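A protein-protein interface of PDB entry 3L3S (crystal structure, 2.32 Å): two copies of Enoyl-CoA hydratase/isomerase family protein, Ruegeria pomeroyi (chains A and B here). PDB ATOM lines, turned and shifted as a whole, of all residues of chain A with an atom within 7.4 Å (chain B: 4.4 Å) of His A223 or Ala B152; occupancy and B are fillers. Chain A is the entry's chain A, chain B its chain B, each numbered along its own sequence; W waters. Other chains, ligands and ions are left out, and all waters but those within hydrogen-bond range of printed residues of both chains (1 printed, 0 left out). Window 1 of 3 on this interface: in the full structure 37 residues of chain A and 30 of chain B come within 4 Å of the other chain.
Water W1 bridges NE of Arg B157 (2.6 Å) and N of Leu A228 (3.5 Å).
OG of Ser B156 is in hydrogen-bond range of NH1 of Arg B157 (3.3 Å).
The side-chain hydroxyl of Ser B156 lies within hydrogen-bond range of the backbone carbonyl oxygen of Val B153.
O of Ala B152 is in hydrogen-bond range of OG of Ser B156 (2.8 Å).
No position is printed for both chains.
Of the 17 pairs that touch across the chains among the printed residues, none has its exchanged pair printed and touching as well.
O of Leu A226 sits at hydrogen-bond distance from NH2 of Arg B157, at 2.6 Å.
The backbone carbonyl oxygen of His A223 lies within hydrogen-bond range of the guanidinium group of Arg B157 (2.9 Å).
Of chain B, only Ala B152, Val B153, Ser B156 and Arg B157 come within 4 Å of His A223.
Ala B152 touches just one residue of chain A: His A223 (3.9 Å).
Of the printed residues of chain B, Ala A235 touches Thr B149, Thr B150 and Val B153.
Of the printed residues of chain B, Ala A231 touches Arg B157 (3.8 Å).
Of the printed residues of chain B, Leu A228 touches Val B153.
Of the printed residues of chain A, Thr B150 touches Tyr A232 (3.9 Å) and Ala A235 (3.9 Å).
Of the printed residues of chain B, Thr A219 touches Thr B149 (3.8 Å).
Arg A222 touches none of the printed residues of chain B.
The nearest residue of chain A that does not touch Ala B152 is Leu A220 (4.3 Å).
Hydrophobic or aromatic side chains of chain A that line the printed part of chain B: His A223, Leu A224, Leu A228, Ala A231, Tyr A232 and Ala A235.
Hydrophobic or aromatic side chains of chain B within 4 Å of the printed part of chain A: Val B153 and Ala B154.
Among the printed residues, 17 pairs touch across the chains.
Among the printed residues, no Asp or Glu carboxylate lies within 4 Å of a Lys or Arg side-chain nitrogen of the other chain.
His A223 touches Ala B152.
Val B153 touches His A223.
His A223 touches Ser B156.
C of Pro A227 touches NH2 of Arg B157, 3.9 Å away.
Val B153 touches Leu A228 (CG1 to CD2, 3.8 Å).
CB of Ala A231 touches NH2 of Arg B157, 3.8 Å away.
CE1 of Tyr A232 touches O of Thr B150 (3.9 Å).
CB of Ala B154 touches OH of Tyr A232 (3.7 Å).
Thr B150 touches Ala A235 (CG2 to O, 3.9 Å).
CG2 of Val B153 touches CB of Ala A235, 3.8 Å away.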
ATOM      1  N   GLY A 216     -17.440  -0.140  26.177  1.00  0.00           N
ATOM      2  CA  GLY A 216     -17.019  -0.680  24.899  1.00  0.00           C
ATOM      3  C   GLY A 216     -17.599  -2.056  24.621  1.00  0.00           C
ATOM      4  O   GLY A 216     -17.994  -2.338  23.486  1.00  0.00           O
ATOM      5  N   LEU A 217     -17.653  -2.900  25.656  1.00  0.00           N
ATOM      6  CA  LEU A 217     -18.190  -4.267  25.563  1.00  0.00           C
ATOM      7  C   LEU A 217     -19.710  -4.230  25.379  1.00  0.00           C
ATOM      8  O   LEU A 217     -20.268  -5.030  24.624  1.00  0.00           O
ATOM      9  CB  LEU A 217     -17.847  -5.069  26.823  1.00  0.00           C
ATOM     10  CG  LEU A 217     -17.537  -6.577  26.860  1.00  0.00           C
ATOM     11  CD1 LEU A 217     -18.200  -7.164  28.096  1.00  0.00           C
ATOM     12  CD2 LEU A 217     -17.967  -7.350  25.620  1.00  0.00           C
ATOM     13  N   GLU A 218     -20.360  -3.276  26.050  1.00  0.00           N
ATOM     14  CA  GLU A 218     -21.811  -3.078  25.964  1.00  0.00           C
ATOM     15  C   GLU A 218     -22.151  -2.713  24.519  1.00  0.00           C
ATOM     16  O   GLU A 218     -23.100  -3.261  23.952  1.00  0.00           O
ATOM     17  CB  GLU A 218     -22.242  -1.948  26.909  1.00  0.00           C
ATOM     18  CG  GLU A 218     -23.746  -1.673  27.012  1.00  0.00           C
ATOM     19  CD  GLU A 218     -24.081  -0.469  27.901  1.00  0.00           C
ATOM     20  OE1 GLU A 218     -25.289  -0.186  28.074  1.00  0.00           O
ATOM     21  OE2 GLU A 218     -23.153   0.196  28.425  1.00  0.00           O
ATOM     22  N   THR A 219     -21.292  -1.874  23.921  1.00  0.00           N
ATOM     23  CA  THR A 219     -21.426  -1.396  22.545  1.00  0.00           C
ATOM     24  C   THR A 219     -21.144  -2.491  21.503  1.00  0.00           C
ATOM     25  O   THR A 219     -21.853  -2.569  20.491  1.00  0.00           O
ATOM     26  CB  THR A 219     -20.524  -0.154  22.291  1.00  0.00           C
ATOM     27  OG1 THR A 219     -20.837   0.853  23.253  1.00  0.00           O
ATOM     28  CG2 THR A 219     -20.753   0.445  20.897  1.00  0.00           C
ATOM     29  N   LEU A 220     -20.137  -3.337  21.766  1.00  0.00           N
ATOM     30  CA  LEU A 220     -19.780  -4.442  20.863  1.00  0.00           C
ATOM     31  C   LEU A 220     -20.939  -5.436  20.743  1.00  0.00           C
ATOM     32  O   LEU A 220     -21.293  -5.829  19.639  1.00  0.00           O
ATOM     33  CB  LEU A 220     -18.485  -5.160  21.306  1.00  0.00           C
ATOM     34  CG  LEU A 220     -18.017  -6.471  20.619  1.00  0.00           C
ATOM     35  CD1 LEU A 220     -17.722  -6.258  19.150  1.00  0.00           C
ATOM     36  CD2 LEU A 220     -16.775  -7.017  21.299  1.00  0.00           C
ATOM     37  N   ASN A 221     -21.565  -5.752  21.877  1.00  0.00           N
ATOM     38  CA  ASN A 221     -22.691  -6.681  21.934  1.00  0.00           C
ATOM     39  C   ASN A 221     -23.903  -6.221  21.131  1.00  0.00           C
ATOM     40  O   ASN A 221     -24.480  -7.017  20.386  1.00  0.00           O
ATOM     41  CB  ASN A 221     -23.119  -6.941  23.382  1.00  0.00           C
ATOM     42  CG  ASN A 221     -22.118  -7.780  24.156  1.00  0.00           C
ATOM     43  OD1 ASN A 221     -21.404  -8.615  23.590  1.00  0.00           O
ATOM     44  ND2 ASN A 221     -22.076  -7.574  25.468  1.00  0.00           N
ATOM     45  N   ARG A 222     -24.251  -4.937  21.238  1.00  0.00           N
ATOM     46  CA  ARG A 222     -25.408  -4.421  20.510  1.00  0.00           C
ATOM     47  C   ARG A 222     -25.168  -4.012  19.066  1.00  0.00           C
ATOM     48  O   ARG A 222     -26.111  -4.040  18.272  1.00  0.00           O
ATOM     49  CB  ARG A 222     -26.157  -3.326  21.287  1.00  0.00           C
ATOM     50  CG  ARG A 222     -25.326  -2.154  21.743  1.00  0.00           C
ATOM     51  CD  ARG A 222     -26.153  -1.104  22.479  1.00  0.00           C
ATOM     52  NE  ARG A 222     -26.838  -1.631  23.653  1.00  0.00           N
ATOM     53  CZ  ARG A 222     -26.978  -0.981  24.804  1.00  0.00           C
ATOM     54  NH1 ARG A 222     -26.465   0.235  24.966  1.00  0.00           N
ATOM     55  NH2 ARG A 222     -27.692  -1.529  25.780  1.00  0.00           N
ATOM     56  N   HIS A 223     -23.926  -3.670  18.706  1.00  0.00           N
ATOM     57  CA  HIS A 223     -23.652  -3.286  17.321  1.00  0.00           C
ATOM     58  C   HIS A 223     -23.547  -4.495  16.385  1.00  0.00           C
ATOM     59  O   HIS A 223     -23.679  -4.368  15.166  1.00  0.00           O
ATOM     60  CB  HIS A 223     -22.492  -2.270  17.194  1.00  0.00           C
ATOM     61  CG  HIS A 223     -21.114  -2.866  17.177  1.00  0.00           C
ATOM     62  ND1 HIS A 223     -20.788  -4.004  16.469  1.00  0.00           N
ATOM     63  CD2 HIS A 223     -19.967  -2.446  17.757  1.00  0.00           C
ATOM     64  CE1 HIS A 223     -19.503  -4.261  16.615  1.00  0.00           C
ATOM     65  NE2 HIS A 223     -18.981  -3.330  17.393  1.00  0.00           N
ATOM     66  N   LEU A 224     -23.331  -5.667  16.992  1.00  0.00           N
ATOM     67  CA  LEU A 224     -23.242  -6.941  16.286  1.00  0.00           C
ATOM     68  C   LEU A 224     -24.621  -7.362  15.770  1.00  0.00           C
ATOM     69  O   LEU A 224     -24.727  -8.182  14.851  1.00  0.00           O
ATOM     70  CB  LEU A 224     -22.695  -8.018  17.220  1.00  0.00           C
ATOM     71  CG  LEU A 224     -21.190  -8.292  17.152  1.00  0.00           C
ATOM     72  CD1 LEU A 224     -20.713  -8.914  18.449  1.00  0.00           C
ATOM     73  CD2 LEU A 224     -20.879  -9.185  15.959  1.00  0.00           C
ATOM     74  N   GLU A 225     -25.658  -6.765  16.368  1.00  0.00           N
ATOM     75  CA  GLU A 225     -27.061  -7.005  16.026  1.00  0.00           C
ATOM     76  C   GLU A 225     -27.631  -5.830  15.221  1.00  0.00           C
ATOM     77  O   GLU A 225     -28.847  -5.619  15.191  1.00  0.00           O
ATOM     78  CB  GLU A 225     -27.880  -7.204  17.310  1.00  0.00           C
ATOM     79  CG  GLU A 225     -27.325  -8.284  18.252  1.00  0.00           C
ATOM     80  CD  GLU A 225     -28.247  -8.618  19.411  1.00  0.00           C
ATOM     81  OE1 GLU A 225     -28.936  -7.706  19.928  1.00  0.00           O
ATOM     82  OE2 GLU A 225     -28.275  -9.806  19.805  1.00  0.00           O
ATOM     83  N   LEU A 226     -26.744  -5.076  14.566  1.00  0.00           N
ATOM     84  CA  LEU A 226     -27.111  -3.897  13.772  1.00  0.00           C
ATOM     85  C   LEU A 226     -26.444  -3.858  12.386  1.00  0.00           C
ATOM     86  O   LEU A 226     -25.465  -4.575  12.153  1.00  0.00           O
ATOM     87  CB  LEU A 226     -26.682  -2.624  14.526  1.00  0.00           C
ATOM     88  CG  LEU A 226     -27.350  -2.132  15.812  1.00  0.00           C
ATOM     89  CD1 LEU A 226     -26.616  -0.902  16.346  1.00  0.00           C
ATOM     90  CD2 LEU A 226     -28.805  -1.830  15.571  1.00  0.00           C
ATOM     91  N   PRO A 227     -27.029  -3.111  11.411  1.00  0.00           N
ATOM     92  CA  PRO A 227     -26.370  -3.048  10.093  1.00  0.00           C
ATOM     93  C   PRO A 227     -25.135  -2.126  10.223  1.00  0.00           C
ATOM     94  O   PRO A 227     -25.064  -1.355  11.193  1.00  0.00           O
ATOM     95  CB  PRO A 227     -27.460  -2.456   9.177  1.00  0.00           C
ATOM     96  CG  PRO A 227     -28.404  -1.770  10.090  1.00  0.00           C
ATOM     97  CD  PRO A 227     -28.440  -2.686  11.290  1.00  0.00           C
ATOM     98  N   LEU A 228     -24.181  -2.201   9.283  1.00  0.00           N
ATOM     99  CA  LEU A 228     -22.937  -1.402   9.337  1.00  0.00           C
ATOM    100  C   LEU A 228     -23.050   0.080   9.671  1.00  0.00           C
ATOM    101  O   LEU A 228     -22.434   0.533  10.630  1.00  0.00           O
ATOM    102  CB  LEU A 228     -22.093  -1.550   8.057  1.00  0.00           C
ATOM    103  CG  LEU A 228     -20.692  -2.201   8.118  1.00  0.00           C
ATOM    104  CD1 LEU A 228     -19.869  -1.712   6.940  1.00  0.00           C
ATOM    105  CD2 LEU A 228     -19.934  -1.898   9.406  1.00  0.00           C
ATOM    106  N   GLN A 230     -25.570   1.841  10.939  1.00  0.00           N
ATOM    107  CA  GLN A 230     -26.171   2.085  12.247  1.00  0.00           C
ATOM    108  C   GLN A 230     -25.210   1.742  13.384  1.00  0.00           C
ATOM    109  O   GLN A 230     -25.223   2.389  14.430  1.00  0.00           O
ATOM    110  CB  GLN A 230     -27.483   1.304  12.393  1.00  0.00           C
ATOM    111  CG  GLN A 230     -28.687   1.926  11.646  1.00  0.00           C
ATOM    112  CD  GLN A 230     -29.281   3.164  12.342  1.00  0.00           C
ATOM    113  OE1 GLN A 230     -29.994   3.951  11.717  1.00  0.00           O
ATOM    114  NE2 GLN A 230     -29.021   3.311  13.643  1.00  0.00           N
ATOM    115  N   ALA A 231     -24.352   0.750  13.149  1.00  0.00           N
ATOM    116  CA  ALA A 231     -23.348   0.319  14.128  1.00  0.00           C
ATOM    117  C   ALA A 231     -22.284   1.404  14.289  1.00  0.00           C
ATOM    118  O   ALA A 231     -21.823   1.665  15.400  1.00  0.00           O
ATOM    119  CB  ALA A 231     -22.716  -0.990  13.696  1.00  0.00           C
ATOM    120  N   TYR A 232     -21.967   2.076  13.178  1.00  0.00           N
ATOM    121  CA  TYR A 232     -20.999   3.165  13.170  1.00  0.00           C
ATOM    122  C   TYR A 232     -21.584   4.420  13.802  1.00  0.00           C
ATOM    123  O   TYR A 232     -20.847   5.232  14.333  1.00  0.00           O
ATOM    124  CB  TYR A 232     -20.477   3.454  11.753  1.00  0.00           C
ATOM    125  CG  TYR A 232     -19.195   2.717  11.398  1.00  0.00           C
ATOM    126  CD1 TYR A 232     -18.067   2.743  12.265  1.00  0.00           C
ATOM    127  CD2 TYR A 232     -19.086   2.005  10.197  1.00  0.00           C
ATOM    128  CE1 TYR A 232     -16.861   2.069  11.934  1.00  0.00           C
ATOM    129  CE2 TYR A 232     -17.888   1.328   9.845  1.00  0.00           C
ATOM    130  CZ  TYR A 232     -16.786   1.365  10.721  1.00  0.00           C
ATOM    131  OH  TYR A 232     -15.641   0.698  10.389  1.00  0.00           O
ATOM    132  N   LEU A 234     -23.680   4.339  16.459  1.00  0.00           N
ATOM    133  CA  LEU A 234     -23.703   4.064  17.889  1.00  0.00           C
ATOM    134  C   LEU A 234     -22.289   4.034  18.479  1.00  0.00           C
ATOM    135  O   LEU A 234     -22.060   4.554  19.574  1.00  0.00           O
ATOM    136  CB  LEU A 234     -24.412   2.733  18.148  1.00  0.00           C
ATOM    137  CG  LEU A 234     -24.509   2.145  19.560  1.00  0.00           C
ATOM    138  CD1 LEU A 234     -25.366   2.983  20.489  1.00  0.00           C
ATOM    139  CD2 LEU A 234     -25.088   0.765  19.431  1.00  0.00           C
ATOM    140  N   ALA A 235     -21.350   3.472  17.717  1.00  0.00           N
ATOM    141  CA  ALA A 235     -19.957   3.323  18.142  1.00  0.00           C
ATOM    142  C   ALA A 235     -19.071   4.567  18.156  1.00  0.00           C
ATOM    143  O   ALA A 235     -18.226   4.695  19.032  1.00  0.00           O
ATOM    144  CB  ALA A 235     -19.291   2.209  17.357  1.00  0.00           C
ATOM    145  N   OCS B 148     -11.017  -0.456  21.780  1.00  0.00           N
ATOM    146  CA  OCS B 148     -11.137  -0.208  20.328  1.00  0.00           C
ATOM    147  CB  OCS B 148     -10.151  -1.054  19.544  1.00  0.00           C
ATOM    148  SG  OCS B 148      -8.518  -0.396  19.710  1.00  0.00           S
ATOM    149  C   OCS B 148     -12.549  -0.431  19.819  1.00  0.00           C
ATOM    150  O   OCS B 148     -12.812  -1.382  19.070  1.00  0.00           O
ATOM    151  OD1 OCS B 148      -7.800  -1.479  19.398  1.00  0.00           O
ATOM    152  OD2 OCS B 148      -8.175   0.639  18.682  1.00  0.00           O
ATOM    153  OD3 OCS B 148      -8.335   0.150  20.905  1.00  0.00           O
ATOM    154  N   THR B 149     -13.426   0.510  20.170  1.00  0.00           N
ATOM    155  CA  THR B 149     -14.834   0.448  19.780  1.00  0.00           C
ATOM    156  C   THR B 149     -15.053   0.546  18.276  1.00  0.00           C
ATOM    157  O   THR B 149     -15.619  -0.386  17.681  1.00  0.00           O
ATOM    158  CB  THR B 149     -15.674   1.443  20.605  1.00  0.00           C
ATOM    159  OG1 THR B 149     -15.595   1.059  21.986  1.00  0.00           O
ATOM    160  CG2 THR B 149     -17.128   1.423  20.219  1.00  0.00           C
ATOM    161  N   THR B 150     -14.560   1.620  17.653  1.00  0.00           N
ATOM    162  CA  THR B 150     -14.733   1.771  16.202  1.00  0.00           C
ATOM    163  C   THR B 150     -13.984   0.703  15.391  1.00  0.00           C
ATOM    164  O   THR B 150     -14.552   0.179  14.453  1.00  0.00           O
ATOM    165  CB  THR B 150     -14.501   3.235  15.698  1.00  0.00           C
ATOM    166  OG1 THR B 150     -13.263   3.760  16.194  1.00  0.00           O
ATOM    167  CG2 THR B 150     -15.636   4.134  16.129  1.00  0.00           C
ATOM    168  N   PRO B 151     -12.723   0.335  15.771  1.00  0.00           N
ATOM    169  CA  PRO B 151     -12.078  -0.706  14.967  1.00  0.00           C
ATOM    170  C   PRO B 151     -12.721  -2.078  15.091  1.00  0.00           C
ATOM    171  O   PRO B 151     -12.702  -2.841  14.126  1.00  0.00           O
ATOM    172  CB  PRO B 151     -10.638  -0.686  15.472  1.00  0.00           C
ATOM    173  CG  PRO B 151     -10.443   0.714  15.803  1.00  0.00           C
ATOM    174  CD  PRO B 151     -11.681   1.019  16.571  1.00  0.00           C
ATOM    175  N   ALA B 152     -13.374  -2.337  16.232  1.00  0.00           N
ATOM    176  CA  ALA B 152     -14.044  -3.624  16.453  1.00  0.00           C
ATOM    177  C   ALA B 152     -15.322  -3.794  15.619  1.00  0.00           C
ATOM    178  O   ALA B 152     -15.816  -4.912  15.467  1.00  0.00           O
ATOM    179  CB  ALA B 152     -14.330  -3.862  17.930  1.00  0.00           C
ATOM    180  N   VAL B 153     -15.817  -2.687  15.050  1.00  0.00           N
ATOM    181  CA  VAL B 153     -17.000  -2.696  14.188  1.00  0.00           C
ATOM    182  C   VAL B 153     -16.676  -3.430  12.881  1.00  0.00           C
ATOM    183  O   VAL B 153     -17.351  -4.402  12.539  1.00  0.00           O
ATOM    184  CB  VAL B 153     -17.523  -1.258  13.909  1.00  0.00           C
ATOM    185  CG1 VAL B 153     -18.662  -1.260  12.893  1.00  0.00           C
ATOM    186  CG2 VAL B 153     -18.006  -0.628  15.188  1.00  0.00           C
ATOM    187  N   ALA B 154     -15.616  -3.000  12.204  1.00  0.00           N
ATOM    188  CA  ALA B 154     -15.196  -3.622  10.953  1.00  0.00           C
ATOM    189  C   ALA B 154     -14.614  -5.018  11.180  1.00  0.00           C
ATOM    190  O   ALA B 154     -14.873  -5.921  10.382  1.00  0.00           O
ATOM    191  CB  ALA B 154     -14.198  -2.738  10.216  1.00  0.00           C
ATOM    192  N   VAL B 155     -13.884  -5.196  12.290  1.00  0.00           N
ATOM    193  CA  VAL B 155     -13.278  -6.489  12.654  1.00  0.00           C
ATOM    194  C   VAL B 155     -14.354  -7.548  12.983  1.00  0.00           C
ATOM    195  O   VAL B 155     -14.242  -8.694  12.543  1.00  0.00           O
ATOM    196  CB  VAL B 155     -12.248  -6.354  13.836  1.00  0.00           C
ATOM    197  CG1 VAL B 155     -11.629  -7.700  14.184  1.00  0.00           C
ATOM    198  CG2 VAL B 155     -11.128  -5.403  13.460  1.00  0.00           C
ATOM    199  N   SER B 156     -15.410  -7.134  13.693  1.00  0.00           N
ATOM    200  CA  SER B 156     -16.520  -8.023  14.063  1.00  0.00           C
ATOM    201  C   SER B 156     -17.302  -8.565  12.873  1.00  0.00           C
ATOM    202  O   SER B 156     -18.079  -9.505  13.016  1.00  0.00           O
ATOM    203  CB  SER B 156     -17.482  -7.329  15.013  1.00  0.00           C
ATOM    204  OG  SER B 156     -18.057  -6.189  14.393  1.00  0.00           O
ATOM    205  N   ARG B 157     -17.098  -7.956  11.705  1.00  0.00           N
ATOM    206  CA  ARG B 157     -17.766  -8.398  10.497  1.00  0.00           C
ATOM    207  C   ARG B 157     -16.977  -9.450   9.739  1.00  0.00           C
ATOM    208  O   ARG B 157     -17.547 -10.161   8.909  1.00  0.00           O
ATOM    209  CB  ARG B 157     -18.115  -7.210   9.594  1.00  0.00           C
ATOM    210  CG  ARG B 157     -19.569  -6.713   9.744  1.00  0.00           C
ATOM    211  CD  ARG B 157     -19.872  -6.223  11.153  1.00  0.00           C
ATOM    212  NE  ARG B 157     -21.186  -5.600  11.267  1.00  0.00           N
ATOM    213  CZ  ARG B 157     -21.674  -5.041  12.377  1.00  0.00           C
ATOM    214  NH1 ARG B 157     -20.967  -5.015  13.505  1.00  0.00           N
ATOM    215  NH2 ARG B 157     -22.882  -4.494  12.353  1.00  0.00           N
ATOM    216  N   VAL B 164     -13.227 -11.751  18.096  1.00  0.00           N
ATOM    217  CA  VAL B 164     -13.211 -10.288  18.303  1.00  0.00           C
ATOM    218  C   VAL B 164     -13.262  -9.921  19.773  1.00  0.00           C
ATOM    219  O   VAL B 164     -12.702  -8.906  20.177  1.00  0.00           O
ATOM    220  CB  VAL B 164     -14.427  -9.545  17.708  1.00  0.00           C
ATOM    221  CG1 VAL B 164     -13.990  -8.212  17.134  1.00  0.00           C
ATOM    222  CG2 VAL B 164     -15.188 -10.380  16.739  1.00  0.00           C
HETATM  223  O   HOH W   1     -22.930  -5.420   9.280  1.00  0.00           O
